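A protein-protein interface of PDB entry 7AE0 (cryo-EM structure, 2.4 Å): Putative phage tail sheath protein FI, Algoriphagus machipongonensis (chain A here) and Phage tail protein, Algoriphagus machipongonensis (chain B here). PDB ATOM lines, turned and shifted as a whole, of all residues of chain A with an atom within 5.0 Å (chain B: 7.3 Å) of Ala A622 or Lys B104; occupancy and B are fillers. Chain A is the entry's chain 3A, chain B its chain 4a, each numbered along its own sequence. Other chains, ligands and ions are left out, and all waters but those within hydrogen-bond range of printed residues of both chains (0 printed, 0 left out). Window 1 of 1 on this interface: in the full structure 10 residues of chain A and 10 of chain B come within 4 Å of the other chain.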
ATOM      1  N   VAL A 618     -17.391  -8.229  25.935  1.00  0.00           N
ATOM      2  CA  VAL A 618     -17.317  -7.606  24.625  1.00  0.00           C
ATOM      3  C   VAL A 618     -16.122  -6.664  24.501  1.00  0.00           C
ATOM      4  O   VAL A 618     -15.417  -6.709  23.490  1.00  0.00           O
ATOM      5  CB  VAL A 618     -18.623  -6.859  24.299  1.00  0.00           C
ATOM      6  CG1 VAL A 618     -18.477  -6.043  23.024  1.00  0.00           C
ATOM      7  CG2 VAL A 618     -19.725  -7.868  24.123  1.00  0.00           C
ATOM      8  N   ARG A 619     -15.895  -5.806  25.499  1.00  0.00           N
ATOM      9  CA  ARG A 619     -14.750  -4.856  25.425  1.00  0.00           C
ATOM     10  C   ARG A 619     -13.420  -5.612  25.335  1.00  0.00           C
ATOM     11  O   ARG A 619     -12.600  -5.221  24.519  1.00  0.00           O
ATOM     12  CB  ARG A 619     -14.740  -3.891  26.616  1.00  0.00           C
ATOM     13  CG  ARG A 619     -15.997  -3.051  26.748  1.00  0.00           C
ATOM     14  CD  ARG A 619     -15.796  -1.653  27.287  1.00  0.00           C
ATOM     15  NE  ARG A 619     -15.567  -1.507  28.715  1.00  0.00           N
ATOM     16  CZ  ARG A 619     -14.455  -1.054  29.270  1.00  0.00           C
ATOM     17  NH1 ARG A 619     -13.431  -0.709  28.516  1.00  0.00           N
ATOM     18  NH2 ARG A 619     -14.365  -0.950  30.582  1.00  0.00           N
ATOM     19  N   VAL A 620     -13.242  -6.689  26.100  1.00  0.00           N
ATOM     20  CA  VAL A 620     -11.992  -7.431  26.094  1.00  0.00           C
ATOM     21  C   VAL A 620     -11.768  -8.087  24.747  1.00  0.00           C
ATOM     22  O   VAL A 620     -10.668  -8.014  24.192  1.00  0.00           O
ATOM     23  CB  VAL A 620     -11.957  -8.480  27.222  1.00  0.00           C
ATOM     24  CG1 VAL A 620     -10.727  -9.383  27.087  1.00  0.00           C
ATOM     25  CG2 VAL A 620     -11.905  -7.760  28.550  1.00  0.00           C
ATOM     26  N   ARG A 621     -12.800  -8.741  24.223  1.00  0.00           N
ATOM     27  CA  ARG A 621     -12.693  -9.382  22.934  1.00  0.00           C
ATOM     28  C   ARG A 621     -12.313  -8.409  21.836  1.00  0.00           C
ATOM     29  O   ARG A 621     -11.412  -8.687  21.042  1.00  0.00           O
ATOM     30  CB  ARG A 621     -13.986 -10.055  22.556  1.00  0.00           C
ATOM     31  CG  ARG A 621     -13.957 -10.683  21.200  1.00  0.00           C
ATOM     32  CD  ARG A 621     -15.151 -11.412  20.900  1.00  0.00           C
ATOM     33  NE  ARG A 621     -15.171 -11.743  19.511  1.00  0.00           N
ATOM     34  CZ  ARG A 621     -16.121 -12.408  18.868  1.00  0.00           C
ATOM     35  NH1 ARG A 621     -17.182 -12.883  19.491  1.00  0.00           N
ATOM     36  NH2 ARG A 621     -15.955 -12.565  17.577  1.00  0.00           N
ATOM     37  N   ALA A 622     -12.997  -7.271  21.768  1.00  0.00           N
ATOM     38  CA  ALA A 622     -12.710  -6.319  20.715  1.00  0.00           C
ATOM     39  C   ALA A 622     -11.269  -5.829  20.760  1.00  0.00           C
ATOM     40  O   ALA A 622     -10.615  -5.724  19.719  1.00  0.00           O
ATOM     41  CB  ALA A 622     -13.656  -5.151  20.835  1.00  0.00           C
ATOM     42  N   MET A 623     -10.751  -5.578  21.962  1.00  0.00           N
ATOM     43  CA  MET A 623      -9.386  -5.118  22.119  1.00  0.00           C
ATOM     44  C   MET A 623      -8.366  -6.133  21.586  1.00  0.00           C
ATOM     45  O   MET A 623      -7.436  -5.768  20.846  1.00  0.00           O
ATOM     46  CB  MET A 623      -9.156  -4.793  23.585  1.00  0.00           C
ATOM     47  CG  MET A 623      -7.784  -4.294  23.937  1.00  0.00           C
ATOM     48  SD  MET A 623      -6.605  -5.605  24.175  1.00  0.00           S
ATOM     49  CE  MET A 623      -7.092  -6.352  25.690  1.00  0.00           C
ATOM     50  N   ILE A 624      -8.556  -7.408  21.931  1.00  0.00           N
ATOM     51  CA  ILE A 624      -7.642  -8.449  21.497  1.00  0.00           C
ATOM     52  C   ILE A 624      -7.674  -8.609  19.980  1.00  0.00           C
ATOM     53  O   ILE A 624      -6.617  -8.762  19.355  1.00  0.00           O
ATOM     54  CB  ILE A 624      -7.927  -9.784  22.196  1.00  0.00           C
ATOM     55  CG1 ILE A 624      -7.611  -9.613  23.689  1.00  0.00           C
ATOM     56  CG2 ILE A 624      -7.042 -10.908  21.570  1.00  0.00           C
ATOM     57  CD1 ILE A 624      -8.094 -10.703  24.575  1.00  0.00           C
ATOM     58  N   GLU A 625      -8.870  -8.624  19.384  1.00  0.00           N
ATOM     59  CA  GLU A 625      -8.951  -8.759  17.941  1.00  0.00           C
ATOM     60  C   GLU A 625      -8.250  -7.606  17.225  1.00  0.00           C
ATOM     61  O   GLU A 625      -7.558  -7.847  16.241  1.00  0.00           O
ATOM     62  CB  GLU A 625     -10.400  -8.830  17.470  1.00  0.00           C
ATOM     63  CG  GLU A 625     -11.147 -10.118  17.796  1.00  0.00           C
ATOM     64  CD  GLU A 625     -12.597 -10.033  17.381  1.00  0.00           C
ATOM     65  OE1 GLU A 625     -13.044  -8.942  17.153  1.00  0.00           O
ATOM     66  OE2 GLU A 625     -13.251 -11.054  17.259  1.00  0.00           O
ATOM     67  N   ASN A 626      -8.363  -6.366  17.723  1.00  0.00           N
ATOM     68  CA  ASN A 626      -7.689  -5.264  17.041  1.00  0.00           C
ATOM     69  C   ASN A 626      -6.170  -5.460  17.017  1.00  0.00           C
ATOM     70  O   ASN A 626      -5.524  -5.227  15.986  1.00  0.00           O
ATOM     71  CB  ASN A 626      -8.057  -3.949  17.678  1.00  0.00           C
ATOM     72  CG  ASN A 626      -9.458  -3.521  17.352  1.00  0.00           C
ATOM     73  OD1 ASN A 626     -10.067  -3.967  16.379  1.00  0.00           O
ATOM     74  ND2 ASN A 626      -9.988  -2.649  18.153  1.00  0.00           N
ATOM     75  N   LEU B  27     -21.657   5.383  11.010  1.00  0.00           N
ATOM     76  CA  LEU B  27     -21.187   3.992  10.972  1.00  0.00           C
ATOM     77  C   LEU B  27     -21.421   3.311   9.607  1.00  0.00           C
ATOM     78  O   LEU B  27     -22.188   2.354   9.495  1.00  0.00           O
ATOM     79  CB  LEU B  27     -21.892   3.233  12.098  1.00  0.00           C
ATOM     80  CG  LEU B  27     -21.665   3.770  13.554  1.00  0.00           C
ATOM     81  CD1 LEU B  27     -22.570   3.050  14.537  1.00  0.00           C
ATOM     82  CD2 LEU B  27     -20.215   3.565  13.968  1.00  0.00           C
ATOM     83  N   ASP B  87      -9.280   2.386  20.845  1.00  0.00           N
ATOM     84  CA  ASP B  87     -10.230   1.408  20.352  1.00  0.00           C
ATOM     85  C   ASP B  87     -11.602   1.887  20.809  1.00  0.00           C
ATOM     86  O   ASP B  87     -11.830   2.087  22.005  1.00  0.00           O
ATOM     87  CB  ASP B  87      -9.928   0.019  20.910  1.00  0.00           C
ATOM     88  CG  ASP B  87      -8.553  -0.482  20.516  1.00  0.00           C
ATOM     89  OD1 ASP B  87      -7.857   0.220  19.753  1.00  0.00           O
ATOM     90  OD2 ASP B  87      -8.170  -1.584  20.965  1.00  0.00           O
ATOM     91  N   LEU B  88     -12.504   2.071  19.860  1.00  0.00           N
ATOM     92  CA  LEU B  88     -13.844   2.585  20.113  1.00  0.00           C
ATOM     93  C   LEU B  88     -14.904   1.484  20.007  1.00  0.00           C
ATOM     94  O   LEU B  88     -15.032   0.835  18.965  1.00  0.00           O
ATOM     95  CB  LEU B  88     -14.103   3.731  19.122  1.00  0.00           C
ATOM     96  CG  LEU B  88     -15.499   4.373  19.027  1.00  0.00           C
ATOM     97  CD1 LEU B  88     -15.847   5.103  20.305  1.00  0.00           C
ATOM     98  CD2 LEU B  88     -15.531   5.314  17.828  1.00  0.00           C
ATOM     99  N   THR B  89     -15.670   1.255  21.075  1.00  0.00           N
ATOM    100  CA  THR B  89     -16.704   0.217  21.011  1.00  0.00           C
ATOM    101  C   THR B  89     -18.103   0.794  21.232  1.00  0.00           C
ATOM    102  O   THR B  89     -18.410   1.364  22.285  1.00  0.00           O
ATOM    103  CB  THR B  89     -16.439  -0.933  21.996  1.00  0.00           C
ATOM    104  OG1 THR B  89     -15.171  -1.526  21.717  1.00  0.00           O
ATOM    105  CG2 THR B  89     -17.488  -2.008  21.828  1.00  0.00           C
ATOM    106  N   ILE B  90     -18.967   0.608  20.246  1.00  0.00           N
ATOM    107  CA  ILE B  90     -20.322   1.146  20.287  1.00  0.00           C
ATOM    108  C   ILE B  90     -21.341   0.014  20.362  1.00  0.00           C
ATOM    109  O   ILE B  90     -21.331  -0.907  19.544  1.00  0.00           O
ATOM    110  CB  ILE B  90     -20.566   2.082  19.088  1.00  0.00           C
ATOM    111  CG1 ILE B  90     -19.564   3.268  19.170  1.00  0.00           C
ATOM    112  CG2 ILE B  90     -22.024   2.568  19.071  1.00  0.00           C
ATOM    113  CD1 ILE B  90     -19.453   4.126  17.945  1.00  0.00           C
ATOM    114  N   THR B 102     -23.034  -4.874  18.166  1.00  0.00           N
ATOM    115  CA  THR B 102     -21.810  -4.135  18.455  1.00  0.00           C
ATOM    116  C   THR B 102     -21.034  -3.706  17.209  1.00  0.00           C
ATOM    117  O   THR B 102     -20.796  -4.489  16.283  1.00  0.00           O
ATOM    118  CB  THR B 102     -20.883  -4.932  19.401  1.00  0.00           C
ATOM    119  OG1 THR B 102     -21.560  -5.187  20.634  1.00  0.00           O
ATOM    120  CG2 THR B 102     -19.618  -4.136  19.721  1.00  0.00           C
ATOM    121  N   TRP B 103     -20.612  -2.449  17.218  1.00  0.00           N
ATOM    122  CA  TRP B 103     -19.773  -1.873  16.182  1.00  0.00           C
ATOM    123  C   TRP B 103     -18.364  -1.679  16.740  1.00  0.00           C
ATOM    124  O   TRP B 103     -18.158  -0.938  17.707  1.00  0.00           O
ATOM    125  CB  TRP B 103     -20.344  -0.540  15.697  1.00  0.00           C
ATOM    126  CG  TRP B 103     -21.670  -0.621  14.984  1.00  0.00           C
ATOM    127  CD1 TRP B 103     -21.880  -0.670  13.648  1.00  0.00           C
ATOM    128  CD2 TRP B 103     -22.968  -0.617  15.585  1.00  0.00           C
ATOM    129  NE1 TRP B 103     -23.212  -0.713  13.382  1.00  0.00           N
ATOM    130  CE2 TRP B 103     -23.899  -0.677  14.557  1.00  0.00           C
ATOM    131  CE3 TRP B 103     -23.420  -0.564  16.894  1.00  0.00           C
ATOM    132  CZ2 TRP B 103     -25.255  -0.689  14.798  1.00  0.00           C
ATOM    133  CZ3 TRP B 103     -24.756  -0.572  17.138  1.00  0.00           C
ATOM    134  CH2 TRP B 103     -25.661  -0.634  16.116  1.00  0.00           C
ATOM    135  N   LYS B 104     -17.398  -2.362  16.151  1.00  0.00           N
ATOM    136  CA  LYS B 104     -16.018  -2.308  16.617  1.00  0.00           C
ATOM    137  C   LYS B 104     -15.141  -1.441  15.720  1.00  0.00           C
ATOM    138  O   LYS B 104     -14.978  -1.739  14.536  1.00  0.00           O
ATOM    139  CB  LYS B 104     -15.461  -3.718  16.687  1.00  0.00           C
ATOM    140  CG  LYS B 104     -16.171  -4.580  17.690  1.00  0.00           C
ATOM    141  CD  LYS B 104     -15.619  -5.969  17.702  1.00  0.00           C
ATOM    142  CE  LYS B 104     -16.312  -6.813  18.731  1.00  0.00           C
ATOM    143  NZ  LYS B 104     -15.773  -8.193  18.758  1.00  0.00           N
ATOM    144  N   VAL B 105     -14.552  -0.381  16.282  1.00  0.00           N
ATOM    145  CA  VAL B 105     -13.761   0.576  15.512  1.00  0.00           C
ATOM    146  C   VAL B 105     -12.282   0.634  15.928  1.00  0.00           C
ATOM    147  O   VAL B 105     -11.938   0.881  17.090  1.00  0.00           O
ATOM    148  CB  VAL B 105     -14.421   1.962  15.588  1.00  0.00           C
ATOM    149  CG1 VAL B 105     -13.597   2.989  14.872  1.00  0.00           C
ATOM    150  CG2 VAL B 105     -15.788   1.889  14.968  1.00  0.00           C
ATOM    151  N   LYS B 106     -11.415   0.446  14.937  1.00  0.00           N
ATOM    152  CA  LYS B 106      -9.955   0.411  15.064  1.00  0.00           C
ATOM    153  C   LYS B 106      -9.242   1.773  14.899  1.00  0.00           C
ATOM    154  O   LYS B 106      -9.490   2.500  13.939  1.00  0.00           O
ATOM    155  CB  LYS B 106      -9.454  -0.561  13.993  1.00  0.00           C
ATOM    156  CG  LYS B 106      -7.983  -0.837  13.950  1.00  0.00           C
ATOM    157  CD  LYS B 106      -7.658  -1.973  12.964  1.00  0.00           C
ATOM    158  CE  LYS B 106      -7.879  -1.541  11.502  1.00  0.00           C
ATOM    159  NZ  LYS B 106      -7.414  -2.546  10.534  1.00  0.00           N
ATOM    160  N   HIS B 134     -10.793   7.055  11.674  1.00  0.00           N
ATOM    161  CA  HIS B 134     -10.465   5.693  12.105  1.00  0.00           C
ATOM    162  C   HIS B 134      -9.992   4.865  10.919  1.00  0.00           C
ATOM    163  O   HIS B 134     -10.003   5.332   9.783  1.00  0.00           O
ATOM    164  CB  HIS B 134     -11.650   5.037  12.800  1.00  0.00           C
ATOM    165  CG  HIS B 134     -12.806   4.811  11.921  1.00  0.00           C
ATOM    166  ND1 HIS B 134     -13.018   3.629  11.247  1.00  0.00           N
ATOM    167  CD2 HIS B 134     -13.798   5.640  11.568  1.00  0.00           C
ATOM    168  CE1 HIS B 134     -14.115   3.746  10.530  1.00  0.00           C
ATOM    169  NE2 HIS B 134     -14.596   4.964  10.699  1.00  0.00           N
ATOM    170  N   GLY B 136     -11.070   1.360  10.316  1.00  0.00           N
ATOM    171  CA  GLY B 136     -11.791   0.125  10.061  1.00  0.00           C
ATOM    172  C   GLY B 136     -12.912  -0.187  11.029  1.00  0.00           C
ATOM    173  O   GLY B 136     -12.828   0.075  12.230  1.00  0.00           O
ATOM    174  N   LEU B 137     -13.954  -0.820  10.484  1.00  0.00           N
ATOM    175  CA  LEU B 137     -15.177  -1.166  11.194  1.00  0.00           C
ATOM    176  C   LEU B 137     -15.646  -2.602  10.952  1.00  0.00           C
ATOM    177  O   LEU B 137     -15.793  -3.039   9.809  1.00  0.00           O
ATOM    178  CB  LEU B 137     -16.290  -0.176  10.792  1.00  0.00           C
ATOM    179  CG  LEU B 137     -17.742  -0.469  11.252  1.00  0.00           C
ATOM    180  CD1 LEU B 137     -17.853  -0.418  12.754  1.00  0.00           C
ATOM    181  CD2 LEU B 137     -18.700   0.560  10.621  1.00  0.00           C
ATOM    182  N   VAL B 138     -15.925  -3.307  12.048  1.00  0.00           N
ATOM    183  CA  VAL B 138     -16.471  -4.665  12.040  1.00  0.00           C
ATOM    184  C   VAL B 138     -17.818  -4.697  12.774  1.00  0.00           C
ATOM    185  O   VAL B 138     -17.957  -4.125  13.860  1.00  0.00           O
ATOM    186  CB  VAL B 138     -15.479  -5.669  12.662  1.00  0.00           C
ATOM    187  CG1 VAL B 138     -16.079  -7.062  12.731  1.00  0.00           C
ATOM    188  CG2 VAL B 138     -14.219  -5.706  11.832  1.00  0.00           C
ATOM    189  N   ILE B 139     -18.822  -5.339  12.180  1.00  0.00           N
ATOM    190  CA  ILE B 139     -20.152  -5.387  12.794  1.00  0.00           C
ATOM    191  C   ILE B 139     -20.499  -6.781  13.309  1.00  0.00           C
ATOM    192  O   ILE B 139     -20.510  -7.752  12.548  1.00  0.00           O
ATOM    193  CB  ILE B 139     -21.232  -4.917  11.814  1.00  0.00           C
ATOM    194  CG1 ILE B 139     -20.894  -3.494  11.353  1.00  0.00           C
ATOM    195  CG2 ILE B 139     -22.613  -4.947  12.525  1.00  0.00           C
ATOM    196  CD1 ILE B 139     -21.710  -2.967  10.210  1.00  0.00           C
ATOM    197  N   GLN B 140     -20.827  -6.875  14.596  1.00  0.00           N
ATOM    198  CA  GLN B 140     -21.175  -8.140  15.237  1.00  0.00           C
ATOM    199  C   GLN B 140     -22.630  -8.199  15.714  1.00  0.00           C
ATOM    200  O   GLN B 140     -23.074  -7.381  16.525  1.00  0.00           O
ATOM    201  CB  GLN B 140     -20.251  -8.395  16.423  1.00  0.00           C
ATOM    202  CG  GLN B 140     -20.495  -9.713  17.143  1.00  0.00           C
ATOM    203  CD  GLN B 140     -19.582  -9.898  18.326  1.00  0.00           C
ATOM    204  OE1 GLN B 140     -19.183  -8.930  18.970  1.00  0.00           O
ATOM    205  NE2 GLN B 140     -19.236 -11.138  18.622  1.00  0.00           N
ATOM    206  N   GLU B 142     -24.971 -11.514  16.808  1.00  0.00           N
ATOM    207  CA  GLU B 142     -25.093 -12.950  16.915  1.00  0.00           C
ATOM    208  C   GLU B 142     -26.411 -13.353  17.564  1.00  0.00           C
ATOM    209  O   GLU B 142     -26.528 -14.427  18.152  1.00  0.00           O
ATOM    210  CB  GLU B 142     -23.919 -13.530  17.704  1.00  0.00           C
ATOM    211  CG  GLU B 142     -22.565 -13.245  17.065  1.00  0.00           C
ATOM    212  CD  GLU B 142     -21.397 -13.775  17.852  1.00  0.00           C
ATOM    213  OE1 GLU B 142     -21.597 -14.314  18.923  1.00  0.00           O
ATOM    214  OE2 GLU B 142     -20.272 -13.534  17.438  1.00  0.00           O
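Of the printed residues of chain B, Glu A625 touches Lys B104 (3.3 Å).
Of the printed residues of chain B, Asn A626 touches Asp B87.
Of the printed residues of chain A, Glu B142 touches Arg A621 (3.8 Å).
Gly B136 touches none of the printed residues of chain A.
Trp B103 touches none of the printed residues of chain A.
The nearest residue of chain B that does not touch Ala A622 is Thr B89 (4.03 Å).
The nearest residue of chain A that does not touch Lys B104 is Val A618 (4.8 Å).
The nearest printed residue of chain A that does not touch Thr B102 is Ala A622 (6.1 Å).
The guanidinium group (NH1) of Arg A621 lies close to the side-chain amide nitrogen (NE2) of Gln B140, at 2.8 Å.
OE2 of Glu B142 is in salt-bridge range of NH1 of Arg A621 (3.8 Å).
The side-chain carboxylate (OE1) of Glu A625 is in salt-bridge range of the side-chain amino group (NZ) of Lys B104, at 3.3 Å.
The side-chain carboxylate (OE2) of Glu A625 is in salt-bridge range of the guanidinium group (NE) of Arg A621, 3.0 Å away.
N of Gln B140 lies within hydrogen-bond range of O of Thr B102 (2.9 Å).
N of Lys B104 is in hydrogen-bond range of O of Val B138.
NZ of Lys B104 sits at hydrogen-bond distance from OE1 of Gln B140 (3.5 Å).
The side-chain amide nitrogen (NE2) of Gln B140 sits at hydrogen-bond distance from the side-chain carboxylate (OE2) of Glu B142, 2.9 Å away.
Among the printed residues, merely in contact across the chains: Asn A626 with Asp B87, Arg A621 with Lys B104, Ala A622 with Lys B104, Met A623 with Asp B87 and Val A618 with Thr B102.
Printed residues of chain B that touch a printed residue of chain A: Asp B87, Thr B102, Lys B104, Gln B140 and Glu B142.
Hydrophobic or aromatic side chains of chain A within 4 Å of the printed part of chain B: Val A618 and Ala A622.
Among the printed residues, Asp or Glu carboxylates within 4 Å of a Lys or Arg side-chain nitrogen of the other chain: Arg A621 with Glu B142 (3.8 Å) and Glu A625 with Lys B104 (3.3 Å).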
